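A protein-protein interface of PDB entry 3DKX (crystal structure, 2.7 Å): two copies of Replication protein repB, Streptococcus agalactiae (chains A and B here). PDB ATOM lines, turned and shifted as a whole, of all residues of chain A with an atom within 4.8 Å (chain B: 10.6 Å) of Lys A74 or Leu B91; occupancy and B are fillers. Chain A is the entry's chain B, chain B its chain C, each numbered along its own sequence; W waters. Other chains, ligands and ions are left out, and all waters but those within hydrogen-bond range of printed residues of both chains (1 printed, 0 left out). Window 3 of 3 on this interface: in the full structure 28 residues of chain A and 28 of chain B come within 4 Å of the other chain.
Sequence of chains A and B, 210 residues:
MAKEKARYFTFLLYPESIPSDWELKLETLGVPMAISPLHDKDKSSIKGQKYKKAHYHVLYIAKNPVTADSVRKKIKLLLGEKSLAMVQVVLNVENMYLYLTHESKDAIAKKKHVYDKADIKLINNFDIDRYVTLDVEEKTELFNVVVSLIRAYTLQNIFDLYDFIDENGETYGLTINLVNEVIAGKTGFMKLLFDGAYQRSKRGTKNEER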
ATOM      1  N   LEU A  29      -0.680  25.875 -14.485  1.00  0.00           N
ATOM      2  CA  LEU A  29      -0.630  27.040 -15.355  1.00  0.00           C
ATOM      3  C   LEU A  29       0.487  26.949 -16.381  1.00  0.00           C
ATOM      4  O   LEU A  29       0.564  27.761 -17.288  1.00  0.00           O
ATOM      5  CB  LEU A  29      -0.433  28.305 -14.525  1.00  0.00           C
ATOM      6  CG  LEU A  29      -1.623  28.670 -13.660  1.00  0.00           C
ATOM      7  CD1 LEU A  29      -1.461  30.063 -13.173  1.00  0.00           C
ATOM      8  CD2 LEU A  29      -2.877  28.557 -14.474  1.00  0.00           C
ATOM      9  N   TYR A  60       6.828  35.179 -10.655  1.00  0.00           N
ATOM     10  CA  TYR A  60       6.024  34.588 -11.725  1.00  0.00           C
ATOM     11  C   TYR A  60       6.472  35.097 -13.098  1.00  0.00           C
ATOM     12  O   TYR A  60       6.399  36.287 -13.381  1.00  0.00           O
ATOM     13  CB  TYR A  60       4.563  34.958 -11.460  1.00  0.00           C
ATOM     14  CG  TYR A  60       3.562  34.552 -12.504  1.00  0.00           C
ATOM     15  CD1 TYR A  60       3.464  35.241 -13.702  1.00  0.00           C
ATOM     16  CD2 TYR A  60       2.674  33.508 -12.277  1.00  0.00           C
ATOM     17  CE1 TYR A  60       2.521  34.884 -14.657  1.00  0.00           C
ATOM     18  CE2 TYR A  60       1.727  33.145 -13.229  1.00  0.00           C
ATOM     19  CZ  TYR A  60       1.657  33.839 -14.415  1.00  0.00           C
ATOM     20  OH  TYR A  60       0.729  33.497 -15.380  1.00  0.00           O
ATOM     21  N   SER A  70      -3.951  40.713 -16.585  1.00  0.00           N
ATOM     22  CA  SER A  70      -4.184  39.404 -17.166  1.00  0.00           C
ATOM     23  C   SER A  70      -3.671  38.349 -16.208  1.00  0.00           C
ATOM     24  O   SER A  70      -4.312  37.321 -15.996  1.00  0.00           O
ATOM     25  CB  SER A  70      -3.514  39.274 -18.538  1.00  0.00           C
ATOM     26  OG  SER A  70      -2.103  39.205 -18.445  1.00  0.00           O
ATOM     27  N   VAL A  71      -2.511  38.615 -15.621  1.00  0.00           N
ATOM     28  CA  VAL A  71      -1.903  37.679 -14.684  1.00  0.00           C
ATOM     29  C   VAL A  71      -2.767  37.569 -13.441  1.00  0.00           C
ATOM     30  O   VAL A  71      -2.911  36.491 -12.880  1.00  0.00           O
ATOM     31  CB  VAL A  71      -0.468  38.085 -14.290  1.00  0.00           C
ATOM     32  CG1 VAL A  71       0.076  37.131 -13.253  1.00  0.00           C
ATOM     33  CG2 VAL A  71       0.438  38.108 -15.502  1.00  0.00           C
ATOM     34  N   ARG A  72      -3.361  38.682 -13.023  1.00  0.00           N
ATOM     35  CA  ARG A  72      -4.195  38.676 -11.829  1.00  0.00           C
ATOM     36  C   ARG A  72      -5.475  37.847 -11.989  1.00  0.00           C
ATOM     37  O   ARG A  72      -5.822  37.062 -11.098  1.00  0.00           O
ATOM     38  CB  ARG A  72      -4.530  40.096 -11.367  1.00  0.00           C
ATOM     39  CG  ARG A  72      -5.492  40.113 -10.193  1.00  0.00           C
ATOM     40  CD  ARG A  72      -5.632  41.486  -9.594  1.00  0.00           C
ATOM     41  NE  ARG A  72      -6.265  42.421 -10.509  1.00  0.00           N
ATOM     42  CZ  ARG A  72      -6.096  43.737 -10.447  1.00  0.00           C
ATOM     43  NH1 ARG A  72      -5.304  44.255  -9.516  1.00  0.00           N
ATOM     44  NH2 ARG A  72      -6.708  44.530 -11.320  1.00  0.00           N
ATOM     45  N   LYS A  73      -6.171  38.020 -13.113  1.00  0.00           N
ATOM     46  CA  LYS A  73      -7.414  37.288 -13.357  1.00  0.00           C
ATOM     47  C   LYS A  73      -7.161  35.800 -13.470  1.00  0.00           C
ATOM     48  O   LYS A  73      -8.001  34.986 -13.106  1.00  0.00           O
ATOM     49  CB  LYS A  73      -8.103  37.800 -14.618  1.00  0.00           C
ATOM     50  CG  LYS A  73      -8.826  39.108 -14.399  1.00  0.00           C
ATOM     51  CD  LYS A  73      -9.135  39.807 -15.703  1.00  0.00           C
ATOM     52  CE  LYS A  73      -9.687  41.199 -15.435  1.00  0.00           C
ATOM     53  NZ  LYS A  73     -10.082  41.874 -16.694  1.00  0.00           N
ATOM     54  N   LYS A  74      -5.986  35.467 -13.983  1.00  0.00           N
ATOM     55  CA  LYS A  74      -5.541  34.097 -14.158  1.00  0.00           C
ATOM     56  C   LYS A  74      -5.386  33.444 -12.795  1.00  0.00           C
ATOM     57  O   LYS A  74      -5.844  32.334 -12.580  1.00  0.00           O
ATOM     58  CB  LYS A  74      -4.204  34.120 -14.902  1.00  0.00           C
ATOM     59  CG  LYS A  74      -3.820  32.899 -15.715  1.00  0.00           C
ATOM     60  CD  LYS A  74      -3.271  33.368 -17.077  1.00  0.00           C
ATOM     61  CE  LYS A  74      -1.977  32.668 -17.505  1.00  0.00           C
ATOM     62  NZ  LYS A  74      -2.172  31.386 -18.241  1.00  0.00           N
ATOM     63  N   ILE A  75      -4.743  34.149 -11.870  1.00  0.00           N
ATOM     64  CA  ILE A  75      -4.526  33.638 -10.515  1.00  0.00           C
ATOM     65  C   ILE A  75      -5.820  33.591  -9.717  1.00  0.00           C
ATOM     66  O   ILE A  75      -6.043  32.677  -8.925  1.00  0.00           O
ATOM     67  CB  ILE A  75      -3.525  34.495  -9.741  1.00  0.00           C
ATOM     68  CG1 ILE A  75      -2.199  34.542 -10.475  1.00  0.00           C
ATOM     69  CG2 ILE A  75      -3.276  33.895  -8.373  1.00  0.00           C
ATOM     70  CD1 ILE A  75      -1.417  33.269 -10.329  1.00  0.00           C
ATOM     71  N   LYS A  76      -6.664  34.592  -9.920  1.00  0.00           N
ATOM     72  CA  LYS A  76      -7.967  34.609  -9.292  1.00  0.00           C
ATOM     73  C   LYS A  76      -8.802  33.401  -9.712  1.00  0.00           C
ATOM     74  O   LYS A  76      -9.318  32.669  -8.877  1.00  0.00           O
ATOM     75  CB  LYS A  76      -8.696  35.898  -9.643  1.00  0.00           C
ATOM     76  CG  LYS A  76      -8.245  37.115  -8.860  1.00  0.00           C
ATOM     77  CD  LYS A  76      -9.397  38.098  -8.792  1.00  0.00           C
ATOM     78  CE  LYS A  76      -9.033  39.397  -8.117  1.00  0.00           C
ATOM     79  NZ  LYS A  76     -10.118  40.385  -8.389  1.00  0.00           N
ATOM     80  N   LEU A  77      -8.938  33.198 -11.013  1.00  0.00           N
ATOM     81  CA  LEU A  77      -9.676  32.059 -11.521  1.00  0.00           C
ATOM     82  C   LEU A  77      -9.130  30.749 -11.017  1.00  0.00           C
ATOM     83  O   LEU A  77      -9.856  29.783 -10.883  1.00  0.00           O
ATOM     84  CB  LEU A  77      -9.636  32.029 -13.040  1.00  0.00           C
ATOM     85  CG  LEU A  77     -10.935  32.386 -13.741  1.00  0.00           C
ATOM     86  CD1 LEU A  77     -11.062  33.898 -13.866  1.00  0.00           C
ATOM     87  CD2 LEU A  77     -10.946  31.715 -15.095  1.00  0.00           C
ATOM     88  N   LEU A  78      -7.834  30.710 -10.771  1.00  0.00           N
ATOM     89  CA  LEU A  78      -7.178  29.486 -10.360  1.00  0.00           C
ATOM     90  C   LEU A  78      -7.440  29.202  -8.878  1.00  0.00           C
ATOM     91  O   LEU A  78      -7.744  28.083  -8.486  1.00  0.00           O
ATOM     92  CB  LEU A  78      -5.681  29.625 -10.597  1.00  0.00           C
ATOM     93  CG  LEU A  78      -4.835  28.396 -10.886  1.00  0.00           C
ATOM     94  CD1 LEU A  78      -3.547  28.458 -10.081  1.00  0.00           C
ATOM     95  CD2 LEU A  78      -5.589  27.138 -10.583  1.00  0.00           C
ATOM     96  N   GLU B   4     -16.493  38.201 -19.039  1.00  0.00           N
ATOM     97  CA  GLU B   4     -15.199  37.555 -19.197  1.00  0.00           C
ATOM     98  C   GLU B   4     -15.135  36.791 -20.503  1.00  0.00           C
ATOM     99  O   GLU B   4     -15.970  35.935 -20.784  1.00  0.00           O
ATOM    100  CB  GLU B   4     -14.864  36.647 -18.011  1.00  0.00           C
ATOM    101  CG  GLU B   4     -14.185  37.406 -16.888  1.00  0.00           C
ATOM    102  CD  GLU B   4     -13.421  38.630 -17.404  1.00  0.00           C
ATOM    103  OE1 GLU B   4     -12.930  38.587 -18.564  1.00  0.00           O
ATOM    104  OE2 GLU B   4     -13.317  39.636 -16.657  1.00  0.00           O
ATOM    105  N   LYS B   5     -14.142  37.126 -21.311  1.00  0.00           N
ATOM    106  CA  LYS B   5     -13.940  36.445 -22.564  1.00  0.00           C
ATOM    107  C   LYS B   5     -12.683  35.608 -22.474  1.00  0.00           C
ATOM    108  O   LYS B   5     -11.796  35.889 -21.675  1.00  0.00           O
ATOM    109  CB  LYS B   5     -13.836  37.454 -23.701  1.00  0.00           C
ATOM    110  CG  LYS B   5     -15.189  37.954 -24.215  1.00  0.00           C
ATOM    111  CD  LYS B   5     -15.028  38.776 -25.499  1.00  0.00           C
ATOM    112  CE  LYS B   5     -16.364  39.044 -26.191  1.00  0.00           C
ATOM    113  NZ  LYS B   5     -16.214  40.052 -27.290  1.00  0.00           N
ATOM    114  N   ALA B   6     -12.615  34.563 -23.286  1.00  0.00           N
ATOM    115  CA  ALA B   6     -11.449  33.694 -23.300  1.00  0.00           C
ATOM    116  C   ALA B   6     -11.352  32.938 -24.620  1.00  0.00           C
ATOM    117  O   ALA B   6     -12.317  32.885 -25.393  1.00  0.00           O
ATOM    118  CB  ALA B   6     -11.486  32.722 -22.119  1.00  0.00           C
ATOM    119  N   ARG B   7     -10.174  32.371 -24.875  1.00  0.00           N
ATOM    120  CA  ARG B   7      -9.953  31.539 -26.048  1.00  0.00           C
ATOM    121  C   ARG B   7     -10.315  30.078 -25.763  1.00  0.00           C
ATOM    122  O   ARG B   7     -11.084  29.467 -26.508  1.00  0.00           O
ATOM    123  CB  ARG B   7      -8.494  31.621 -26.514  1.00  0.00           C
ATOM    124  CG  ARG B   7      -8.111  32.902 -27.271  1.00  0.00           C
ATOM    125  CD  ARG B   7      -7.007  32.637 -28.312  1.00  0.00           C
ATOM    126  NE  ARG B   7      -7.580  32.354 -29.633  1.00  0.00           N
ATOM    127  CZ  ARG B   7      -7.045  31.542 -30.543  1.00  0.00           C
ATOM    128  NH1 ARG B   7      -5.913  30.890 -30.291  1.00  0.00           N
ATOM    129  NH2 ARG B   7      -7.653  31.375 -31.705  1.00  0.00           N
ATOM    130  N   TYR B   8      -9.766  29.532 -24.678  1.00  0.00           N
ATOM    131  CA  TYR B   8      -9.831  28.092 -24.409  1.00  0.00           C
ATOM    132  C   TYR B   8     -10.909  27.699 -23.403  1.00  0.00           C
ATOM    133  O   TYR B   8     -11.023  28.292 -22.331  1.00  0.00           O
ATOM    134  CB  TYR B   8      -8.458  27.584 -23.962  1.00  0.00           C
ATOM    135  CG  TYR B   8      -7.331  28.240 -24.725  1.00  0.00           C
ATOM    136  CD1 TYR B   8      -7.365  28.319 -26.110  1.00  0.00           C
ATOM    137  CD2 TYR B   8      -6.243  28.803 -24.062  1.00  0.00           C
ATOM    138  CE1 TYR B   8      -6.344  28.930 -26.813  1.00  0.00           C
ATOM    139  CE2 TYR B   8      -5.217  29.415 -24.759  1.00  0.00           C
ATOM    140  CZ  TYR B   8      -5.277  29.478 -26.133  1.00  0.00           C
ATOM    141  OH  TYR B   8      -4.269  30.085 -26.838  1.00  0.00           O
ATOM    142  N   PHE B   9     -11.695  26.688 -23.755  1.00  0.00           N
ATOM    143  CA  PHE B   9     -12.795  26.241 -22.903  1.00  0.00           C
ATOM    144  C   PHE B   9     -12.808  24.732 -22.689  1.00  0.00           C
ATOM    145  O   PHE B   9     -12.039  23.995 -23.296  1.00  0.00           O
ATOM    146  CB  PHE B   9     -14.142  26.706 -23.467  1.00  0.00           C
ATOM    147  CG  PHE B   9     -14.290  28.198 -23.519  1.00  0.00           C
ATOM    148  CD1 PHE B   9     -13.706  28.931 -24.541  1.00  0.00           C
ATOM    149  CD2 PHE B   9     -15.001  28.867 -22.541  1.00  0.00           C
ATOM    150  CE1 PHE B   9     -13.830  30.306 -24.584  1.00  0.00           C
ATOM    151  CE2 PHE B   9     -15.129  30.240 -22.576  1.00  0.00           C
ATOM    152  CZ  PHE B   9     -14.542  30.962 -23.598  1.00  0.00           C
ATOM    153  N   THR B  10     -13.685  24.280 -21.807  1.00  0.00           N
ATOM    154  CA  THR B  10     -13.847  22.855 -21.584  1.00  0.00           C
ATOM    155  C   THR B  10     -15.207  22.604 -20.974  1.00  0.00           C
ATOM    156  O   THR B  10     -15.741  23.450 -20.273  1.00  0.00           O
ATOM    157  CB  THR B  10     -12.749  22.277 -20.675  1.00  0.00           C
ATOM    158  OG1 THR B  10     -12.778  20.849 -20.741  1.00  0.00           O
ATOM    159  CG2 THR B  10     -12.950  22.720 -19.235  1.00  0.00           C
ATOM    160  N   LEU B  59     -12.204  19.640 -25.095  1.00  0.00           N
ATOM    161  CA  LEU B  59     -11.319  20.792 -25.118  1.00  0.00           C
ATOM    162  C   LEU B  59     -11.705  21.639 -26.317  1.00  0.00           C
ATOM    163  O   LEU B  59     -11.580  21.191 -27.453  1.00  0.00           O
ATOM    164  CB  LEU B  59      -9.872  20.350 -25.266  1.00  0.00           C
ATOM    165  CG  LEU B  59      -8.790  21.245 -24.652  1.00  0.00           C
ATOM    166  CD1 LEU B  59      -7.414  20.744 -25.024  1.00  0.00           C
ATOM    167  CD2 LEU B  59      -8.940  22.701 -25.006  1.00  0.00           C
ATOM    168  N   TYR B  60     -12.153  22.865 -26.077  1.00  0.00           N
ATOM    169  CA  TYR B  60     -12.763  23.662 -27.133  1.00  0.00           C
ATOM    170  C   TYR B  60     -12.010  24.963 -27.369  1.00  0.00           C
ATOM    171  O   TYR B  60     -11.755  25.713 -26.443  1.00  0.00           O
ATOM    172  CB  TYR B  60     -14.217  23.939 -26.752  1.00  0.00           C
ATOM    173  CG  TYR B  60     -15.012  24.805 -27.696  1.00  0.00           C
ATOM    174  CD1 TYR B  60     -14.812  26.177 -27.740  1.00  0.00           C
ATOM    175  CD2 TYR B  60     -16.004  24.255 -28.507  1.00  0.00           C
ATOM    176  CE1 TYR B  60     -15.555  26.981 -28.584  1.00  0.00           C
ATOM    177  CE2 TYR B  60     -16.762  25.055 -29.363  1.00  0.00           C
ATOM    178  CZ  TYR B  60     -16.531  26.416 -29.391  1.00  0.00           C
ATOM    179  OH  TYR B  60     -17.258  27.222 -30.226  1.00  0.00           O
ATOM    180  N   ILE B  61     -11.677  25.252 -28.619  1.00  0.00           N
ATOM    181  CA  ILE B  61     -10.812  26.387 -28.905  1.00  0.00           C
ATOM    182  C   ILE B  61     -11.416  27.464 -29.796  1.00  0.00           C
ATOM    183  O   ILE B  61     -11.352  27.387 -31.019  1.00  0.00           O
ATOM    184  CB  ILE B  61      -9.525  25.894 -29.529  1.00  0.00           C
ATOM    185  CG1 ILE B  61      -8.706  25.161 -28.458  1.00  0.00           C
ATOM    186  CG2 ILE B  61      -8.774  27.062 -30.146  1.00  0.00           C
ATOM    187  CD1 ILE B  61      -7.960  23.968 -28.987  1.00  0.00           C
ATOM    188  N   GLN B  88     -16.089  25.378 -18.244  1.00  0.00           N
ATOM    189  CA  GLN B  88     -15.082  26.232 -17.609  1.00  0.00           C
ATOM    190  C   GLN B  88     -14.109  26.849 -18.624  1.00  0.00           C
ATOM    191  O   GLN B  88     -13.905  26.314 -19.722  1.00  0.00           O
ATOM    192  CB  GLN B  88     -14.280  25.430 -16.579  1.00  0.00           C
ATOM    193  CG  GLN B  88     -15.020  24.248 -15.962  1.00  0.00           C
ATOM    194  CD  GLN B  88     -14.081  23.270 -15.260  1.00  0.00           C
ATOM    195  OE1 GLN B  88     -13.441  23.609 -14.274  1.00  0.00           O
ATOM    196  NE2 GLN B  88     -14.001  22.054 -15.771  1.00  0.00           N
ATOM    197  N   VAL B  89     -13.495  27.970 -18.253  1.00  0.00           N
ATOM    198  CA  VAL B  89     -12.402  28.503 -19.053  1.00  0.00           C
ATOM    199  C   VAL B  89     -11.125  27.769 -18.707  1.00  0.00           C
ATOM    200  O   VAL B  89     -10.985  27.272 -17.607  1.00  0.00           O
ATOM    201  CB  VAL B  89     -12.223  30.003 -18.882  1.00  0.00           C
ATOM    202  CG1 VAL B  89     -12.938  30.482 -17.647  1.00  0.00           C
ATOM    203  CG2 VAL B  89     -10.754  30.347 -18.852  1.00  0.00           C
ATOM    204  N   VAL B  90     -10.218  27.666 -19.672  1.00  0.00           N
ATOM    205  CA  VAL B  90      -9.018  26.845 -19.519  1.00  0.00           C
ATOM    206  C   VAL B  90      -7.782  27.720 -19.570  1.00  0.00           C
ATOM    207  O   VAL B  90      -7.601  28.510 -20.498  1.00  0.00           O
ATOM    208  CB  VAL B  90      -8.914  25.753 -20.613  1.00  0.00           C
ATOM    209  CG1 VAL B  90      -7.497  25.217 -20.719  1.00  0.00           C
ATOM    210  CG2 VAL B  90      -9.860  24.629 -20.326  1.00  0.00           C
ATOM    211  N   LEU B  91      -6.925  27.580 -18.570  1.00  0.00           N
ATOM    212  CA  LEU B  91      -5.804  28.480 -18.467  1.00  0.00           C
ATOM    213  C   LEU B  91      -4.546  27.891 -19.078  1.00  0.00           C
ATOM    214  O   LEU B  91      -3.672  28.628 -19.504  1.00  0.00           O
ATOM    215  CB  LEU B  91      -5.584  28.901 -17.014  1.00  0.00           C
ATOM    216  CG  LEU B  91      -6.868  29.387 -16.344  1.00  0.00           C
ATOM    217  CD1 LEU B  91      -6.677  29.595 -14.853  1.00  0.00           C
ATOM    218  CD2 LEU B  91      -7.340  30.666 -17.012  1.00  0.00           C
ATOM    219  N   ASN B  92      -4.432  26.574 -19.114  1.00  0.00           N
ATOM    220  CA  ASN B  92      -3.292  25.975 -19.786  1.00  0.00           C
ATOM    221  C   ASN B  92      -3.685  24.810 -20.712  1.00  0.00           C
ATOM    222  O   ASN B  92      -3.849  23.666 -20.266  1.00  0.00           O
ATOM    223  CB  ASN B  92      -2.252  25.540 -18.775  1.00  0.00           C
ATOM    224  CG  ASN B  92      -1.134  24.778 -19.415  1.00  0.00           C
ATOM    225  OD1 ASN B  92      -1.071  24.708 -20.629  1.00  0.00           O
ATOM    226  ND2 ASN B  92      -0.257  24.188 -18.619  1.00  0.00           N
ATOM    227  N   VAL B  93      -3.843  25.118 -21.998  1.00  0.00           N
ATOM    228  CA  VAL B  93      -4.378  24.173 -22.972  1.00  0.00           C
ATOM    229  C   VAL B  93      -3.683  22.833 -22.886  1.00  0.00           C
ATOM    230  O   VAL B  93      -4.318  21.770 -22.877  1.00  0.00           O
ATOM    231  CB  VAL B  93      -4.253  24.696 -24.411  1.00  0.00           C
ATOM    232  CG1 VAL B  93      -4.665  23.620 -25.382  1.00  0.00           C
ATOM    233  CG2 VAL B  93      -5.137  25.932 -24.634  1.00  0.00           C
ATOM    234  N   GLU B  94      -2.369  22.868 -22.800  1.00  0.00           N
ATOM    235  CA  GLU B  94      -1.639  21.626 -22.702  1.00  0.00           C
ATOM    236  C   GLU B  94      -2.032  20.838 -21.457  1.00  0.00           C
ATOM    237  O   GLU B  94      -2.213  19.612 -21.513  1.00  0.00           O
ATOM    238  CB  GLU B  94      -0.138  21.867 -22.716  1.00  0.00           C
ATOM    239  CG  GLU B  94       0.641  20.593 -22.871  1.00  0.00           C
ATOM    240  CD  GLU B  94       2.104  20.769 -22.558  1.00  0.00           C
ATOM    241  OE1 GLU B  94       2.613  21.922 -22.533  1.00  0.00           O
ATOM    242  OE2 GLU B  94       2.752  19.728 -22.330  1.00  0.00           O
ATOM    243  N   ASN B  95      -2.163  21.527 -20.325  1.00  0.00           N
ATOM    244  CA  ASN B  95      -2.552  20.816 -19.116  1.00  0.00           C
ATOM    245  C   ASN B  95      -3.887  20.101 -19.323  1.00  0.00           C
ATOM    246  O   ASN B  95      -4.020  18.897 -19.047  1.00  0.00           O
ATOM    247  CB  ASN B  95      -2.605  21.740 -17.906  1.00  0.00           C
ATOM    248  CG  ASN B  95      -2.839  20.984 -16.619  1.00  0.00           C
ATOM    249  OD1 ASN B  95      -1.944  20.306 -16.104  1.00  0.00           O
ATOM    250  ND2 ASN B  95      -4.053  21.081 -16.097  1.00  0.00           N
ATOM    251  N   MET B  96      -4.865  20.833 -19.847  1.00  0.00           N
ATOM    252  CA  MET B  96      -6.172  20.240 -20.035  1.00  0.00           C
ATOM    253  C   MET B  96      -6.130  19.087 -21.054  1.00  0.00           C
ATOM    254  O   MET B  96      -6.815  18.074 -20.885  1.00  0.00           O
ATOM    255  CB  MET B  96      -7.207  21.292 -20.416  1.00  0.00           C
ATOM    256  CG  MET B  96      -8.551  20.686 -20.766  1.00  0.00           C
ATOM    257  SD  MET B  96      -9.404  19.837 -19.378  1.00  0.00           S
ATOM    258  CE  MET B  96     -10.161  21.273 -18.607  1.00  0.00           C
ATOM    259  N   TYR B  97      -5.308  19.238 -22.102  1.00  0.00           N
ATOM    260  CA  TYR B  97      -5.227  18.210 -23.133  1.00  0.00           C
ATOM    261  C   TYR B  97      -4.684  16.937 -22.534  1.00  0.00           C
ATOM    262  O   TYR B  97      -5.142  15.844 -22.863  1.00  0.00           O
ATOM    263  CB  TYR B  97      -4.349  18.659 -24.304  1.00  0.00           C
ATOM    264  CG  TYR B  97      -4.175  17.621 -25.419  1.00  0.00           C
ATOM    265  CD1 TYR B  97      -5.018  17.622 -26.525  1.00  0.00           C
ATOM    266  CD2 TYR B  97      -3.156  16.660 -25.361  1.00  0.00           C
ATOM    267  CE1 TYR B  97      -4.873  16.690 -27.535  1.00  0.00           C
ATOM    268  CE2 TYR B  97      -2.998  15.721 -26.367  1.00  0.00           C
ATOM    269  CZ  TYR B  97      -3.864  15.744 -27.462  1.00  0.00           C
ATOM    270  OH  TYR B  97      -3.727  14.830 -28.487  1.00  0.00           O
ATOM    271  N   TYR B 131      -0.444  24.428 -29.812  1.00  0.00           N
ATOM    272  CA  TYR B 131      -0.821  25.205 -28.612  1.00  0.00           C
ATOM    273  C   TYR B 131       0.279  25.282 -27.554  1.00  0.00           C
ATOM    274  O   TYR B 131       0.135  25.964 -26.559  1.00  0.00           O
ATOM    275  CB  TYR B 131      -2.126  24.663 -28.020  1.00  0.00           C
ATOM    276  CG  TYR B 131      -3.245  24.881 -28.989  1.00  0.00           C
ATOM    277  CD1 TYR B 131      -3.708  26.159 -29.232  1.00  0.00           C
ATOM    278  CD2 TYR B 131      -3.790  23.827 -29.719  1.00  0.00           C
ATOM    279  CE1 TYR B 131      -4.700  26.396 -30.146  1.00  0.00           C
ATOM    280  CE2 TYR B 131      -4.800  24.053 -30.646  1.00  0.00           C
ATOM    281  CZ  TYR B 131      -5.245  25.352 -30.854  1.00  0.00           C
ATOM    282  OH  TYR B 131      -6.233  25.640 -31.767  1.00  0.00           O
ATOM    283  N   VAL B 132       1.381  24.589 -27.821  1.00  0.00           N
ATOM    284  CA  VAL B 132       2.524  24.486 -26.938  1.00  0.00           C
ATOM    285  C   VAL B 132       3.769  25.000 -27.640  1.00  0.00           C
ATOM    286  O   VAL B 132       3.990  24.738 -28.813  1.00  0.00           O
ATOM    287  CB  VAL B 132       2.788  23.032 -26.601  1.00  0.00           C
ATOM    288  CG1 VAL B 132       4.097  22.898 -25.836  1.00  0.00           C
ATOM    289  CG2 VAL B 132       1.600  22.448 -25.847  1.00  0.00           C
HETATM  290  O   HOH W   1      -4.353  30.975 -20.604  1.00  0.00           O
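1 position is printed for both chains.
Of the 5 pairs that touch across the chains among the printed residues, none has its exchanged pair printed and touching as well.
Leu A29 touches Leu B91 (CD2 to CB, 3.7 Å).
Asn B92 touches Leu A29.
Val B89 touches Leu A77 (CG1 to CD2, 3.5 Å).
Water W1 lies within hydrogen-bond range of the backbone carbonyl oxygen of Leu B91 (2.7 Å) and the side-chain amino group of Lys A74 (3.2 Å).
NZ of Lys A73 is in salt-bridge range of OE2 of Glu B4 (3.9 Å).
The backbone carbonyl oxygen of Leu B91 is in hydrogen-bond range of the side-chain amino group of Lys A74 (3.4 Å).
OD1 of Asn B92 is in hydrogen-bond range of N of Glu B94 (3.1 Å).
OD1 of Asn B92 is in hydrogen-bond range of N of Asn B95 (3.4 Å).
Of chain B, only Leu B91 (3.4 Å) comes within 4 Å of Lys A74.
No residue of chain B comes within 4 Å of Ile A75.
Leu A77 touches one residue of chain B.
No residue of chain B comes within 4 Å of Leu A78.
Of the printed residues of chain B, Lys A73 touches Glu B4.
Printed residues of chain A within 4 Å of Asn B92: Leu A29.
Of the printed residues of chain A, Val B89 touches Leu A77.
Tyr A60 touches none of the printed residues of chain B.
Hydrophobic or aromatic side chains of chain A that line the printed part of chain B: Leu A29 and Leu A77.
Among the printed residues, Asp or Glu carboxylates within 4 Å of a Lys or Arg side-chain nitrogen of the other chain: Lys A73 with Glu B4 (3.9 Å).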
